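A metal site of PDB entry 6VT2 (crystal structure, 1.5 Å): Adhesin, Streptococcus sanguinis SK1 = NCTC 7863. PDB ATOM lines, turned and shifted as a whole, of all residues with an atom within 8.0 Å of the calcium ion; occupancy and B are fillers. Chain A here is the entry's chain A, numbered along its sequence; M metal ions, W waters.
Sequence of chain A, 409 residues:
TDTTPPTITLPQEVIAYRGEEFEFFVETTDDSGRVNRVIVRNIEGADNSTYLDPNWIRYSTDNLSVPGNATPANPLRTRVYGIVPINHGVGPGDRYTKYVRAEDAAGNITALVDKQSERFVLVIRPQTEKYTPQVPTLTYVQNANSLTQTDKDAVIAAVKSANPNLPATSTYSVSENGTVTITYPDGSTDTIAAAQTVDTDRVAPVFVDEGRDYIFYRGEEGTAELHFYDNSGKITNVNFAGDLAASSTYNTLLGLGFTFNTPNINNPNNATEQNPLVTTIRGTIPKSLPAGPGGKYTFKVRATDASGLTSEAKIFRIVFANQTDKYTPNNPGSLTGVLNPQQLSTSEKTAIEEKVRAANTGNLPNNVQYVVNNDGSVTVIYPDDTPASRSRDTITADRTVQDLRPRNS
Within 4 Å of the calcium ion: Thr 324, Tyr 327 and Asp 393.
The backbone carbonyl oxygen of Arg 392 sits close to the side-chain hydroxyl of Thr 324, at 2.7 Å. The side-chain amino group (NZ) of Lys 326 sits at hydrogen-bond distance from the side-chain hydroxyl (OH) of Tyr 327, at 3.4 Å. O of Asp 393 lies within hydrogen-bond range of N of Val 380 (2.8 Å). The side-chain carboxylate (OD2) of Asp 393 lies close to the side-chain hydroxyl (OH) of Tyr 382. OG of Ser 391 is in hydrogen-bond range of N of Thr 324 (3.1 Å).
The calcium ion is bound by water W3 (2.3 Å), O of Thr 324 (2.4 Å), OD2 of Asp 393 (2.4 Å), water W1 (2.4 Å), O of Tyr 327 (2.4 Å), water W2 (2.5 Å), OD1 of Asp 393 (2.5 Å) and OG1 of Thr 324 (2.6 Å).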
ATOM      1  N   ASN A 322      13.190  17.825 -12.394  1.00  0.00           N
ATOM      2  CA  ASN A 322      13.875  18.548 -11.339  1.00  0.00           C
ATOM      3  C   ASN A 322      14.761  19.587 -11.956  1.00  0.00           C
ATOM      4  O   ASN A 322      15.365  19.360 -13.016  1.00  0.00           O
ATOM      5  CB  ASN A 322      14.721  17.616 -10.508  1.00  0.00           C
ATOM      6  CG  ASN A 322      13.933  16.628  -9.760  1.00  0.00           C
ATOM      7  OD1 ASN A 322      12.954  16.947  -9.079  1.00  0.00           O
ATOM      8  ND2 ASN A 322      14.319  15.390  -9.864  1.00  0.00           N
ATOM      9  N   GLN A 323      14.966  20.674 -11.243  1.00  0.00           N
ATOM     10  CA  GLN A 323      15.874  21.701 -11.744  1.00  0.00           C
ATOM     11  C   GLN A 323      17.286  21.198 -11.979  1.00  0.00           C
ATOM     12  O   GLN A 323      17.969  21.698 -12.893  1.00  0.00           O
ATOM     13  CB  GLN A 323      15.904  22.890 -10.796  1.00  0.00           C
ATOM     14  CG  GLN A 323      14.638  23.705 -10.956  1.00  0.00           C
ATOM     15  CD  GLN A 323      14.619  24.919 -10.103  1.00  0.00           C
ATOM     16  OE1 GLN A 323      15.707  25.510  -9.777  1.00  0.00           O
ATOM     17  NE2 GLN A 323      13.432  25.318  -9.661  1.00  0.00           N
ATOM     18  N   THR A 324      17.727  20.252 -11.198  1.00  0.00           N
ATOM     19  CA  THR A 324      19.070  19.763 -11.424  1.00  0.00           C
ATOM     20  C   THR A 324      19.204  19.182 -12.802  1.00  0.00           C
ATOM     21  O   THR A 324      20.314  19.123 -13.319  1.00  0.00           O
ATOM     22  CB  THR A 324      19.479  18.776 -10.337  1.00  0.00           C
ATOM     23  OG1 THR A 324      20.860  18.466 -10.580  1.00  0.00           O
ATOM     24  CG2 THR A 324      18.675  17.515 -10.356  1.00  0.00           C
ATOM     25  N   ASP A 325      18.099  18.793 -13.445  1.00  0.00           N
ATOM     26  CA  ASP A 325      18.200  18.246 -14.779  1.00  0.00           C
ATOM     27  C   ASP A 325      18.572  19.308 -15.806  1.00  0.00           C
ATOM     28  O   ASP A 325      19.053  18.952 -16.890  1.00  0.00           O
ATOM     29  CB  ASP A 325      16.881  17.598 -15.162  1.00  0.00           C
ATOM     30  CG  ASP A 325      16.573  16.368 -14.427  1.00  0.00           C
ATOM     31  OD1 ASP A 325      17.365  15.941 -13.575  1.00  0.00           O
ATOM     32  OD2 ASP A 325      15.448  15.825 -14.654  1.00  0.00           O
ATOM     33  N   LYS A 326      18.379  20.593 -15.517  1.00  0.00           N
ATOM     34  CA  LYS A 326      18.809  21.601 -16.475  1.00  0.00           C
ATOM     35  C   LYS A 326      19.994  22.431 -16.058  1.00  0.00           C
ATOM     36  O   LYS A 326      20.448  23.239 -16.861  1.00  0.00           O
ATOM     37  CB  LYS A 326      17.669  22.549 -16.816  1.00  0.00           C
ATOM     38  CG  LYS A 326      17.189  23.287 -15.678  1.00  0.00           C
ATOM     39  CD  LYS A 326      16.134  24.417 -16.147  1.00  0.00           C
ATOM     40  CE  LYS A 326      16.728  25.583 -16.755  1.00  0.00           C
ATOM     41  NZ  LYS A 326      15.759  26.710 -16.936  1.00  0.00           N
ATOM     42  N   TYR A 327      20.466  22.321 -14.833  1.00  0.00           N
ATOM     43  CA  TYR A 327      21.594  23.100 -14.353  1.00  0.00           C
ATOM     44  C   TYR A 327      22.788  22.210 -14.106  1.00  0.00           C
ATOM     45  O   TYR A 327      22.658  21.148 -13.510  1.00  0.00           O
ATOM     46  CB  TYR A 327      21.234  23.784 -13.000  1.00  0.00           C
ATOM     47  CG  TYR A 327      20.195  24.844 -13.226  1.00  0.00           C
ATOM     48  CD1 TYR A 327      20.453  25.934 -14.055  1.00  0.00           C
ATOM     49  CD2 TYR A 327      18.949  24.764 -12.645  1.00  0.00           C
ATOM     50  CE1 TYR A 327      19.493  26.881 -14.306  1.00  0.00           C
ATOM     51  CE2 TYR A 327      17.995  25.675 -12.913  1.00  0.00           C
ATOM     52  CZ  TYR A 327      18.262  26.758 -13.726  1.00  0.00           C
ATOM     53  OH  TYR A 327      17.294  27.715 -14.018  1.00  0.00           O
ATOM     54  N   THR A 328      23.970  22.694 -14.491  1.00  0.00           N
ATOM     55  CA  THR A 328      25.231  22.043 -14.172  1.00  0.00           C
ATOM     56  C   THR A 328      26.112  23.100 -13.509  1.00  0.00           C
ATOM     57  O   THR A 328      26.405  24.116 -14.155  1.00  0.00           O
ATOM     58  CB  THR A 328      25.883  21.541 -15.445  1.00  0.00           C
ATOM     59  OG1 THR A 328      25.024  20.558 -16.009  1.00  0.00           O
ATOM     60  CG2 THR A 328      27.208  20.915 -15.142  1.00  0.00           C
ATOM     61  N   PRO A 329      26.523  22.869 -12.256  1.00  0.00           N
ATOM     62  CA  PRO A 329      27.430  23.822 -11.609  1.00  0.00           C
ATOM     63  C   PRO A 329      28.748  23.952 -12.359  1.00  0.00           C
ATOM     64  O   PRO A 329      29.292  22.970 -12.860  1.00  0.00           O
ATOM     65  CB  PRO A 329      27.625  23.245 -10.201  1.00  0.00           C
ATOM     66  CG  PRO A 329      26.484  22.323 -10.036  1.00  0.00           C
ATOM     67  CD  PRO A 329      26.100  21.790 -11.340  1.00  0.00           C
ATOM     68  N   LEU A 364      23.585  29.174 -12.286  1.00  0.00           N
ATOM     69  CA  LEU A 364      22.598  28.544 -11.425  1.00  0.00           C
ATOM     70  C   LEU A 364      21.594  29.570 -10.945  1.00  0.00           C
ATOM     71  O   LEU A 364      21.863  30.758 -10.994  1.00  0.00           O
ATOM     72  CB  LEU A 364      23.286  27.921 -10.233  1.00  0.00           C
ATOM     73  CG  LEU A 364      24.387  26.940 -10.596  1.00  0.00           C
ATOM     74  CD1 LEU A 364      25.014  26.359  -9.353  1.00  0.00           C
ATOM     75  CD2 LEU A 364      23.865  25.921 -11.525  1.00  0.00           C
ATOM     76  N   VAL A 380      24.971  21.212  -3.976  1.00  0.00           N
ATOM     77  CA  VAL A 380      24.221  22.290  -4.567  1.00  0.00           C
ATOM     78  C   VAL A 380      22.767  21.869  -4.499  1.00  0.00           C
ATOM     79  O   VAL A 380      22.383  20.830  -5.055  1.00  0.00           O
ATOM     80  CB  VAL A 380      24.658  22.517  -6.007  1.00  0.00           C
ATOM     81  CG1 VAL A 380      23.891  23.610  -6.656  1.00  0.00           C
ATOM     82  CG2 VAL A 380      26.159  22.805  -6.090  1.00  0.00           C
ATOM     83  N   TYR A 382      18.955  22.931  -5.339  1.00  0.00           N
ATOM     84  CA  TYR A 382      18.134  23.797  -6.148  1.00  0.00           C
ATOM     85  C   TYR A 382      16.819  24.009  -5.458  1.00  0.00           C
ATOM     86  O   TYR A 382      16.439  23.246  -4.572  1.00  0.00           O
ATOM     87  CB  TYR A 382      17.888  23.143  -7.503  1.00  0.00           C
ATOM     88  CG  TYR A 382      19.150  22.999  -8.259  1.00  0.00           C
ATOM     89  CD1 TYR A 382      19.688  24.087  -8.924  1.00  0.00           C
ATOM     90  CD2 TYR A 382      19.819  21.793  -8.309  1.00  0.00           C
ATOM     91  CE1 TYR A 382      20.877  23.994  -9.571  1.00  0.00           C
ATOM     92  CE2 TYR A 382      21.001  21.692  -8.991  1.00  0.00           C
ATOM     93  CZ  TYR A 382      21.535  22.775  -9.571  1.00  0.00           C
ATOM     94  OH  TYR A 382      22.740  22.709 -10.229  1.00  0.00           O
ATOM     95  N   SER A 391      16.601  17.595  -5.657  1.00  0.00           N
ATOM     96  CA  SER A 391      17.071  18.341  -6.794  1.00  0.00           C
ATOM     97  C   SER A 391      18.386  18.980  -6.401  1.00  0.00           C
ATOM     98  O   SER A 391      18.416  20.074  -5.826  1.00  0.00           O
ATOM     99  CB  SER A 391      16.045  19.383  -7.203  1.00  0.00           C
ATOM    100  OG  SER A 391      16.433  19.993  -8.404  1.00  0.00           O
ATOM    101  N   ARG A 392      19.466  18.294  -6.764  1.00  0.00           N
ATOM    102  CA  ARG A 392      20.772  18.604  -6.195  1.00  0.00           C
ATOM    103  C   ARG A 392      21.854  18.283  -7.202  1.00  0.00           C
ATOM    104  O   ARG A 392      21.623  17.520  -8.169  1.00  0.00           O
ATOM    105  CB  ARG A 392      21.016  17.818  -4.902  1.00  0.00           C
ATOM    106  CG  ARG A 392      20.038  18.147  -3.831  1.00  0.00           C
ATOM    107  CD  ARG A 392      20.361  17.362  -2.524  1.00  0.00           C
ATOM    108  NE  ARG A 392      19.311  17.697  -1.615  1.00  0.00           N
ATOM    109  CZ  ARG A 392      19.432  17.836  -0.315  1.00  0.00           C
ATOM    110  NH1 ARG A 392      20.618  17.601   0.271  1.00  0.00           N
ATOM    111  NH2 ARG A 392      18.398  18.209   0.381  1.00  0.00           N
ATOM    112  N   ASP A 393      23.041  18.849  -6.966  1.00  0.00           N
ATOM    113  CA  ASP A 393      24.246  18.474  -7.677  1.00  0.00           C
ATOM    114  C   ASP A 393      25.323  18.400  -6.618  1.00  0.00           C
ATOM    115  O   ASP A 393      25.156  18.927  -5.519  1.00  0.00           O
ATOM    116  CB  ASP A 393      24.615  19.466  -8.775  1.00  0.00           C
ATOM    117  CG  ASP A 393      23.839  19.251 -10.064  1.00  0.00           C
ATOM    118  OD1 ASP A 393      23.720  18.092 -10.478  1.00  0.00           O
ATOM    119  OD2 ASP A 393      23.411  20.213 -10.702  1.00  0.00           O
ATOM    120  N   THR A 394      26.397  17.702  -6.947  1.00  0.00           N
ATOM    121  CA  THR A 394      27.553  17.608  -6.062  1.00  0.00           C
ATOM    122  C   THR A 394      28.760  18.109  -6.818  1.00  0.00           C
ATOM    123  O   THR A 394      28.989  17.739  -7.981  1.00  0.00           O
ATOM    124  CB  THR A 394      27.782  16.171  -5.616  1.00  0.00           C
ATOM    125  OG1 THR A 394      26.664  15.717  -4.870  1.00  0.00           O
ATOM    126  CG2 THR A 394      29.088  16.144  -4.709  1.00  0.00           C
HETATM  127 CA    CA M   1      22.561  18.918 -12.559  1.00  0.00          CA
HETATM  128  O   HOH W   1      22.229  16.532 -12.800  1.00  0.00           O
HETATM  129  O   HOH W   2      22.889  18.574 -15.004  1.00  0.00           O
HETATM  130  O   HOH W   3      24.806  18.664 -13.196  1.00  0.00           O
